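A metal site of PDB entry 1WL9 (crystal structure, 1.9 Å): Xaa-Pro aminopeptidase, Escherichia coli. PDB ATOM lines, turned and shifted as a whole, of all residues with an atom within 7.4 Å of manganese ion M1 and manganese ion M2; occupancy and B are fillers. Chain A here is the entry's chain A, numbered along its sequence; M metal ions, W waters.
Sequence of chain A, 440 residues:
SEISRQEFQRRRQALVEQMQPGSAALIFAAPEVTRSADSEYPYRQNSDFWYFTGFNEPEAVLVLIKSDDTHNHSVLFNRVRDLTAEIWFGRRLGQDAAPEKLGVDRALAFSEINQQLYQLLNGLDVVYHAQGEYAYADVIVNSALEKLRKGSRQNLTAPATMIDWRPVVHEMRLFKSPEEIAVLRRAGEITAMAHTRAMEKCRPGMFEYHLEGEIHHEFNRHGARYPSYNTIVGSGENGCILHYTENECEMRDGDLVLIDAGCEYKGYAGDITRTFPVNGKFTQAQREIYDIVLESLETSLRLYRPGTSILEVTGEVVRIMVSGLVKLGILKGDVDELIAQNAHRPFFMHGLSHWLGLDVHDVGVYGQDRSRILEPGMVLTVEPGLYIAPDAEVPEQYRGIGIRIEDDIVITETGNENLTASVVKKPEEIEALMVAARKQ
N of Ala 261 sits close to OH of Tyr 229 (3.0 Å).
The side-chain carboxylate (OE1) of Glu 383 is in salt-bridge range of the guanidinium group (NE) of Arg 404, 3.8 Å away.
The side-chain hydroxyl of Tyr 229 sits close to the side-chain carboxylate of Asp 271 (2.9 Å).
OD2 of Asp 260 lies close to NH2 of Arg 404 (2.8 Å).
The guanidinium group (NE) of Arg 404 is in hydrogen-bond range of the side-chain hydroxyl (OG1) of Thr 273 (3.2 Å).
ND1 of His 354 lies close to O of Val 360, at 2.9 Å.
The side-chain hydroxyl of Thr 381 sits close to the side-chain carboxylate of Glu 383 (3.0 Å).
N of Glu 406 lies within hydrogen-bond range of O of Thr 273, at 2.9 Å.
Merely in contact with manganese ion M1: Thr 381.
Merely in contact with manganese ion M2: Thr 273 (3.5 Å) and Tyr 229 (3.7 Å).
Within 4 Å of manganese ion M2: Tyr 229, Asp 260, Asp 271, Thr 273, Glu 383 and Glu 406.
The nearest printed residue that does not touch manganese ion M2 is Ile 272 (4.7 Å).
Manganese ion M1 is bound by water W1 (2.0 Å), the side-chain carboxylate of Glu 406 (2.1 Å), a ring nitrogen (NE2) of His 354 (2.2 Å), the side-chain carboxylate of Asp 271 (2.2 Å) and the side-chain carboxylate of Glu 383 (2.3 Å).
Manganese ion M1 has five donor atoms within binding distance.
Slightly farther from manganese ion M1 lies water W3 (2.8 Å).
Manganese ion M2 is bound by the side-chain carboxylate (OD1) of Asp 271 (2.1 Å), water W1 (2.1 Å), the side-chain carboxylate (OD1) of Asp 260 (2.2 Å), the side-chain carboxylate (OE1) of Glu 406 (2.2 Å), the side-chain carboxylate (OD2) of Asp 260 (2.3 Å) and water W2 (2.4 Å).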
ATOM      1  N   TYR A 229      17.112  -8.602 -32.244  1.00  0.00           N
ATOM      2  CA  TYR A 229      17.997  -7.581 -32.838  1.00  0.00           C
ATOM      3  C   TYR A 229      18.127  -7.909 -34.311  1.00  0.00           C
ATOM      4  O   TYR A 229      17.766  -8.998 -34.725  1.00  0.00           O
ATOM      5  CB  TYR A 229      19.401  -7.554 -32.201  1.00  0.00           C
ATOM      6  CG  TYR A 229      20.082  -8.905 -32.154  1.00  0.00           C
ATOM      7  CD1 TYR A 229      19.890  -9.780 -31.086  1.00  0.00           C
ATOM      8  CD2 TYR A 229      20.919  -9.319 -33.199  1.00  0.00           C
ATOM      9  CE1 TYR A 229      20.498 -11.003 -31.053  1.00  0.00           C
ATOM     10  CE2 TYR A 229      21.537 -10.570 -33.168  1.00  0.00           C
ATOM     11  CZ  TYR A 229      21.338 -11.399 -32.081  1.00  0.00           C
ATOM     12  OH  TYR A 229      21.972 -12.634 -32.057  1.00  0.00           O
ATOM     13  N   ILE A 232      22.573 -10.570 -38.410  1.00  0.00           N
ATOM     14  CA  ILE A 232      23.837 -10.363 -39.111  1.00  0.00           C
ATOM     15  C   ILE A 232      24.223 -11.643 -39.819  1.00  0.00           C
ATOM     16  O   ILE A 232      24.331 -12.691 -39.174  1.00  0.00           O
ATOM     17  CB  ILE A 232      24.945 -10.048 -38.093  1.00  0.00           C
ATOM     18  CG1 ILE A 232      24.648  -8.702 -37.419  1.00  0.00           C
ATOM     19  CG2 ILE A 232      26.337 -10.063 -38.728  1.00  0.00           C
ATOM     20  CD1 ILE A 232      25.410  -8.514 -36.128  1.00  0.00           C
ATOM     21  N   HIS A 243      28.561  -5.237 -36.877  1.00  0.00           N
ATOM     22  CA  HIS A 243      27.087  -5.286 -37.033  1.00  0.00           C
ATOM     23  C   HIS A 243      26.717  -5.088 -38.518  1.00  0.00           C
ATOM     24  O   HIS A 243      25.991  -4.178 -38.888  1.00  0.00           O
ATOM     25  CB  HIS A 243      26.366  -4.289 -36.111  1.00  0.00           C
ATOM     26  CG  HIS A 243      26.695  -4.457 -34.650  1.00  0.00           C
ATOM     27  ND1 HIS A 243      27.202  -5.628 -34.124  1.00  0.00           N
ATOM     28  CD2 HIS A 243      26.578  -3.601 -33.609  1.00  0.00           C
ATOM     29  CE1 HIS A 243      27.390  -5.482 -32.822  1.00  0.00           C
ATOM     30  NE2 HIS A 243      27.005  -4.265 -32.484  1.00  0.00           N
ATOM     31  N   ILE A 259      27.190 -15.726 -38.618  1.00  0.00           N
ATOM     32  CA  ILE A 259      25.770 -15.465 -38.384  1.00  0.00           C
ATOM     33  C   ILE A 259      25.562 -15.126 -36.915  1.00  0.00           C
ATOM     34  O   ILE A 259      25.849 -15.951 -36.033  1.00  0.00           O
ATOM     35  CB  ILE A 259      24.900 -16.653 -38.756  1.00  0.00           C
ATOM     36  CG1 ILE A 259      25.087 -16.998 -40.245  1.00  0.00           C
ATOM     37  CG2 ILE A 259      23.442 -16.337 -38.472  1.00  0.00           C
ATOM     38  CD1 ILE A 259      24.122 -18.052 -40.734  1.00  0.00           C
ATOM     39  N   ASP A 260      25.058 -13.925 -36.661  1.00  0.00           N
ATOM     40  CA  ASP A 260      24.699 -13.487 -35.323  1.00  0.00           C
ATOM     41  C   ASP A 260      23.207 -13.190 -35.366  1.00  0.00           C
ATOM     42  O   ASP A 260      22.737 -12.277 -36.062  1.00  0.00           O
ATOM     43  CB  ASP A 260      25.528 -12.280 -34.892  1.00  0.00           C
ATOM     44  CG  ASP A 260      25.417 -11.963 -33.417  1.00  0.00           C
ATOM     45  OD1 ASP A 260      24.472 -12.420 -32.728  1.00  0.00           O
ATOM     46  OD2 ASP A 260      26.303 -11.236 -32.909  1.00  0.00           O
ATOM     47  N   ALA A 261      22.435 -14.046 -34.707  1.00  0.00           N
ATOM     48  CA  ALA A 261      20.984 -13.914 -34.711  1.00  0.00           C
ATOM     49  C   ALA A 261      20.379 -14.497 -33.458  1.00  0.00           C
ATOM     50  O   ALA A 261      20.914 -15.443 -32.862  1.00  0.00           O
ATOM     51  CB  ALA A 261      20.384 -14.590 -35.946  1.00  0.00           C
ATOM     52  N   GLY A 262      19.275 -13.895 -33.052  1.00  0.00           N
ATOM     53  CA  GLY A 262      18.608 -14.268 -31.827  1.00  0.00           C
ATOM     54  C   GLY A 262      17.141 -13.960 -31.881  1.00  0.00           C
ATOM     55  O   GLY A 262      16.713 -12.949 -32.461  1.00  0.00           O
ATOM     56  N   GLY A 270      17.228 -14.313 -27.127  1.00  0.00           N
ATOM     57  CA  GLY A 270      18.384 -15.131 -27.461  1.00  0.00           C
ATOM     58  C   GLY A 270      19.431 -14.305 -28.192  1.00  0.00           C
ATOM     59  O   GLY A 270      19.128 -13.246 -28.776  1.00  0.00           O
ATOM     60  N   ASP A 271      20.667 -14.787 -28.195  1.00  0.00           N
ATOM     61  CA  ASP A 271      21.770 -14.099 -28.847  1.00  0.00           C
ATOM     62  C   ASP A 271      22.913 -15.093 -29.116  1.00  0.00           C
ATOM     63  O   ASP A 271      23.744 -15.330 -28.270  1.00  0.00           O
ATOM     64  CB  ASP A 271      22.250 -12.951 -27.953  1.00  0.00           C
ATOM     65  CG  ASP A 271      23.333 -12.111 -28.598  1.00  0.00           C
ATOM     66  OD1 ASP A 271      23.716 -12.368 -29.784  1.00  0.00           O
ATOM     67  OD2 ASP A 271      23.780 -11.172 -27.908  1.00  0.00           O
ATOM     68  N   ILE A 272      22.917 -15.675 -30.314  1.00  0.00           N
ATOM     69  CA  ILE A 272      23.910 -16.664 -30.717  1.00  0.00           C
ATOM     70  C   ILE A 272      24.664 -16.189 -31.930  1.00  0.00           C
ATOM     71  O   ILE A 272      24.082 -15.617 -32.877  1.00  0.00           O
ATOM     72  CB  ILE A 272      23.250 -18.008 -31.046  1.00  0.00           C
ATOM     73  CG1 ILE A 272      22.618 -18.646 -29.797  1.00  0.00           C
ATOM     74  CG2 ILE A 272      24.262 -18.968 -31.723  1.00  0.00           C
ATOM     75  CD1 ILE A 272      22.017 -19.981 -30.068  1.00  0.00           C
ATOM     76  N   THR A 273      25.982 -16.388 -31.884  1.00  0.00           N
ATOM     77  CA  THR A 273      26.803 -16.253 -33.075  1.00  0.00           C
ATOM     78  C   THR A 273      27.462 -17.617 -33.365  1.00  0.00           C
ATOM     79  O   THR A 273      28.004 -18.283 -32.469  1.00  0.00           O
ATOM     80  CB  THR A 273      27.901 -15.169 -32.968  1.00  0.00           C
ATOM     81  OG1 THR A 273      27.363 -13.901 -32.540  1.00  0.00           O
ATOM     82  CG2 THR A 273      28.550 -14.966 -34.309  1.00  0.00           C
ATOM     83  N   GLY A 351      33.762  -6.228 -26.208  1.00  0.00           N
ATOM     84  CA  GLY A 351      33.662  -6.917 -24.933  1.00  0.00           C
ATOM     85  C   GLY A 351      33.358  -8.390 -25.104  1.00  0.00           C
ATOM     86  O   GLY A 351      32.762  -8.812 -26.112  1.00  0.00           O
ATOM     87  N   LEU A 352      33.802  -9.177 -24.127  1.00  0.00           N
ATOM     88  CA  LEU A 352      33.573 -10.623 -24.126  1.00  0.00           C
ATOM     89  C   LEU A 352      32.123 -10.986 -23.799  1.00  0.00           C
ATOM     90  O   LEU A 352      31.597 -11.988 -24.270  1.00  0.00           O
ATOM     91  CB  LEU A 352      34.492 -11.305 -23.097  1.00  0.00           C
ATOM     92  CG  LEU A 352      34.387 -12.834 -22.966  1.00  0.00           C
ATOM     93  CD1 LEU A 352      34.848 -13.508 -24.260  1.00  0.00           C
ATOM     94  CD2 LEU A 352      35.173 -13.354 -21.775  1.00  0.00           C
ATOM     95  N   SER A 353      31.482 -10.179 -22.954  1.00  0.00           N
ATOM     96  CA  SER A 353      30.190 -10.554 -22.398  1.00  0.00           C
ATOM     97  C   SER A 353      29.343  -9.343 -22.111  1.00  0.00           C
ATOM     98  O   SER A 353      29.850  -8.330 -21.642  1.00  0.00           O
ATOM     99  CB  SER A 353      30.411 -11.306 -21.086  1.00  0.00           C
ATOM    100  OG  SER A 353      31.060 -12.553 -21.265  1.00  0.00           O
ATOM    101  N   HIS A 354      28.047  -9.455 -22.366  1.00  0.00           N
ATOM    102  CA  HIS A 354      27.069  -8.478 -21.906  1.00  0.00           C
ATOM    103  C   HIS A 354      25.920  -9.228 -21.237  1.00  0.00           C
ATOM    104  O   HIS A 354      25.658 -10.393 -21.536  1.00  0.00           O
ATOM    105  CB  HIS A 354      26.562  -7.591 -23.028  1.00  0.00           C
ATOM    106  CG  HIS A 354      25.940  -8.343 -24.158  1.00  0.00           C
ATOM    107  ND1 HIS A 354      24.634  -8.787 -24.136  1.00  0.00           N
ATOM    108  CD2 HIS A 354      26.447  -8.728 -25.350  1.00  0.00           C
ATOM    109  CE1 HIS A 354      24.380  -9.431 -25.259  1.00  0.00           C
ATOM    110  NE2 HIS A 354      25.460  -9.400 -26.015  1.00  0.00           N
ATOM    111  N   TRP A 355      25.259  -8.572 -20.315  1.00  0.00           N
ATOM    112  CA  TRP A 355      24.023  -9.092 -19.738  1.00  0.00           C
ATOM    113  C   TRP A 355      22.982  -9.329 -20.835  1.00  0.00           C
ATOM    114  O   TRP A 355      22.956  -8.625 -21.865  1.00  0.00           O
ATOM    115  CB  TRP A 355      23.381  -8.140 -18.729  1.00  0.00           C
ATOM    116  CG  TRP A 355      24.264  -7.522 -17.697  1.00  0.00           C
ATOM    117  CD1 TRP A 355      24.368  -6.195 -17.438  1.00  0.00           C
ATOM    118  CD2 TRP A 355      25.122  -8.185 -16.736  1.00  0.00           C
ATOM    119  NE1 TRP A 355      25.253  -5.970 -16.404  1.00  0.00           N
ATOM    120  CE2 TRP A 355      25.721  -7.171 -15.948  1.00  0.00           C
ATOM    121  CE3 TRP A 355      25.424  -9.524 -16.465  1.00  0.00           C
ATOM    122  CZ2 TRP A 355      26.615  -7.453 -14.902  1.00  0.00           C
ATOM    123  CZ3 TRP A 355      26.333  -9.810 -15.435  1.00  0.00           C
ATOM    124  CH2 TRP A 355      26.912  -8.781 -14.658  1.00  0.00           C
ATOM    125  N   LEU A 356      22.081 -10.267 -20.554  1.00  0.00           N
ATOM    126  CA  LEU A 356      21.038 -10.694 -21.473  1.00  0.00           C
ATOM    127  C   LEU A 356      19.690 -10.823 -20.749  1.00  0.00           C
ATOM    128  O   LEU A 356      19.611 -11.322 -19.602  1.00  0.00           O
ATOM    129  CB  LEU A 356      21.443 -12.040 -22.070  1.00  0.00           C
ATOM    130  CG  LEU A 356      20.599 -12.614 -23.211  1.00  0.00           C
ATOM    131  CD1 LEU A 356      20.768 -11.794 -24.502  1.00  0.00           C
ATOM    132  CD2 LEU A 356      20.998 -14.037 -23.434  1.00  0.00           C
ATOM    133  N   VAL A 360      18.598  -7.425 -25.476  1.00  0.00           N
ATOM    134  CA  VAL A 360      19.787  -8.185 -25.827  1.00  0.00           C
ATOM    135  C   VAL A 360      21.010  -7.617 -25.146  1.00  0.00           C
ATOM    136  O   VAL A 360      21.813  -8.373 -24.634  1.00  0.00           O
ATOM    137  CB  VAL A 360      19.987  -8.348 -27.357  1.00  0.00           C
ATOM    138  CG1 VAL A 360      20.140  -7.040 -28.069  1.00  0.00           C
ATOM    139  CG2 VAL A 360      21.207  -9.239 -27.644  1.00  0.00           C
ATOM    140  N   HIS A 361      21.154  -6.295 -25.124  1.00  0.00           N
ATOM    141  CA  HIS A 361      22.158  -5.682 -24.236  1.00  0.00           C
ATOM    142  C   HIS A 361      21.422  -5.291 -22.978  1.00  0.00           C
ATOM    143  O   HIS A 361      20.897  -4.184 -22.853  1.00  0.00           O
ATOM    144  CB  HIS A 361      22.862  -4.500 -24.866  1.00  0.00           C
ATOM    145  CG  HIS A 361      23.652  -4.866 -26.069  1.00  0.00           C
ATOM    146  ND1 HIS A 361      23.843  -4.007 -27.122  1.00  0.00           N
ATOM    147  CD2 HIS A 361      24.225  -6.043 -26.425  1.00  0.00           C
ATOM    148  CE1 HIS A 361      24.536  -4.626 -28.068  1.00  0.00           C
ATOM    149  NE2 HIS A 361      24.788  -5.856 -27.659  1.00  0.00           N
ATOM    150  N   THR A 381      26.123 -13.131 -22.109  1.00  0.00           N
ATOM    151  CA  THR A 381      26.673 -13.784 -23.280  1.00  0.00           C
ATOM    152  C   THR A 381      28.157 -14.032 -23.098  1.00  0.00           C
ATOM    153  O   THR A 381      28.793 -13.457 -22.212  1.00  0.00           O
ATOM    154  CB  THR A 381      26.474 -12.932 -24.569  1.00  0.00           C
ATOM    155  OG1 THR A 381      27.197 -11.700 -24.435  1.00  0.00           O
ATOM    156  CG2 THR A 381      25.019 -12.665 -24.793  1.00  0.00           C
ATOM    157  N   VAL A 382      28.693 -14.926 -23.925  1.00  0.00           N
ATOM    158  CA  VAL A 382      30.129 -15.161 -23.990  1.00  0.00           C
ATOM    159  C   VAL A 382      30.458 -15.192 -25.493  1.00  0.00           C
ATOM    160  O   VAL A 382      30.049 -16.115 -26.194  1.00  0.00           O
ATOM    161  CB  VAL A 382      30.519 -16.493 -23.287  1.00  0.00           C
ATOM    162  CG1 VAL A 382      32.046 -16.633 -23.158  1.00  0.00           C
ATOM    163  CG2 VAL A 382      29.831 -16.618 -21.931  1.00  0.00           C
ATOM    164  N   GLU A 383      31.168 -14.185 -25.974  1.00  0.00           N
ATOM    165  CA  GLU A 383      31.311 -13.975 -27.406  1.00  0.00           C
ATOM    166  C   GLU A 383      32.695 -13.472 -27.842  1.00  0.00           C
ATOM    167  O   GLU A 383      32.834 -12.397 -28.413  1.00  0.00           O
ATOM    168  CB  GLU A 383      30.203 -13.063 -27.935  1.00  0.00           C
ATOM    169  CG  GLU A 383      30.058 -11.688 -27.298  1.00  0.00           C
ATOM    170  CD  GLU A 383      28.879 -10.932 -27.884  1.00  0.00           C
ATOM    171  OE1 GLU A 383      28.792 -10.807 -29.134  1.00  0.00           O
ATOM    172  OE2 GLU A 383      28.029 -10.498 -27.100  1.00  0.00           O
ATOM    173  N   ARG A 404      33.383 -14.979 -34.919  1.00  0.00           N
ATOM    174  CA  ARG A 404      32.868 -14.883 -33.564  1.00  0.00           C
ATOM    175  C   ARG A 404      32.055 -16.128 -33.253  1.00  0.00           C
ATOM    176  O   ARG A 404      31.385 -16.711 -34.125  1.00  0.00           O
ATOM    177  CB  ARG A 404      32.041 -13.592 -33.391  1.00  0.00           C
ATOM    178  CG  ARG A 404      31.338 -13.474 -32.070  1.00  0.00           C
ATOM    179  CD  ARG A 404      30.779 -12.064 -31.856  1.00  0.00           C
ATOM    180  NE  ARG A 404      29.653 -11.679 -32.712  1.00  0.00           N
ATOM    181  CZ  ARG A 404      29.709 -10.840 -33.759  1.00  0.00           C
ATOM    182  NH1 ARG A 404      30.836 -10.325 -34.177  1.00  0.00           N
ATOM    183  NH2 ARG A 404      28.606 -10.512 -34.413  1.00  0.00           N
ATOM    184  N   GLU A 406      29.442 -17.312 -30.100  1.00  0.00           N
ATOM    185  CA  GLU A 406      28.732 -16.722 -28.967  1.00  0.00           C
ATOM    186  C   GLU A 406      27.657 -17.654 -28.435  1.00  0.00           C
ATOM    187  O   GLU A 406      26.803 -18.113 -29.205  1.00  0.00           O
ATOM    188  CB  GLU A 406      28.097 -15.391 -29.377  1.00  0.00           C
ATOM    189  CG  GLU A 406      27.068 -14.811 -28.407  1.00  0.00           C
ATOM    190  CD  GLU A 406      26.601 -13.429 -28.839  1.00  0.00           C
ATOM    191  OE1 GLU A 406      26.501 -13.212 -30.051  1.00  0.00           O
ATOM    192  OE2 GLU A 406      26.356 -12.573 -27.959  1.00  0.00           O
ATOM    193  N   ASP A 407      27.716 -17.887 -27.123  1.00  0.00           N
ATOM    194  CA  ASP A 407      26.732 -18.648 -26.369  1.00  0.00           C
ATOM    195  C   ASP A 407      26.118 -17.749 -25.309  1.00  0.00           C
ATOM    196  O   ASP A 407      26.701 -16.737 -24.952  1.00  0.00           O
ATOM    197  CB  ASP A 407      27.383 -19.848 -25.695  1.00  0.00           C
ATOM    198  CG  ASP A 407      27.548 -21.041 -26.645  1.00  0.00           C
ATOM    199  OD1 ASP A 407      26.753 -21.161 -27.601  1.00  0.00           O
ATOM    200  OD2 ASP A 407      28.442 -21.842 -26.373  1.00  0.00           O
ATOM    201  N   ASP A 408      24.947 -18.142 -24.815  1.00  0.00           N
ATOM    202  CA  ASP A 408      24.260 -17.448 -23.722  1.00  0.00           C
ATOM    203  C   ASP A 408      24.275 -18.357 -22.487  1.00  0.00           C
ATOM    204  O   ASP A 408      23.963 -19.564 -22.576  1.00  0.00           O
ATOM    205  CB  ASP A 408      22.810 -17.129 -24.101  1.00  0.00           C
ATOM    206  CG  ASP A 408      22.701 -16.449 -25.428  1.00  0.00           C
ATOM    207  OD1 ASP A 408      23.645 -15.676 -25.758  1.00  0.00           O
ATOM    208  OD2 ASP A 408      21.684 -16.690 -26.129  1.00  0.00           O
HETATM  209 MN    MN M   1      25.888 -10.500 -27.845  1.00  0.00          MN
HETATM  210 MN    MN M   2      25.293 -11.588 -30.887  1.00  0.00          MN
HETATM  211  O   HOH W   1      26.436 -10.154 -29.786  1.00  0.00           O
HETATM  212  O   HOH W   2      24.062  -9.555 -31.064  1.00  0.00           O
HETATM  213  O   HOH W   3      25.248  -7.971 -28.970  1.00  0.00           O
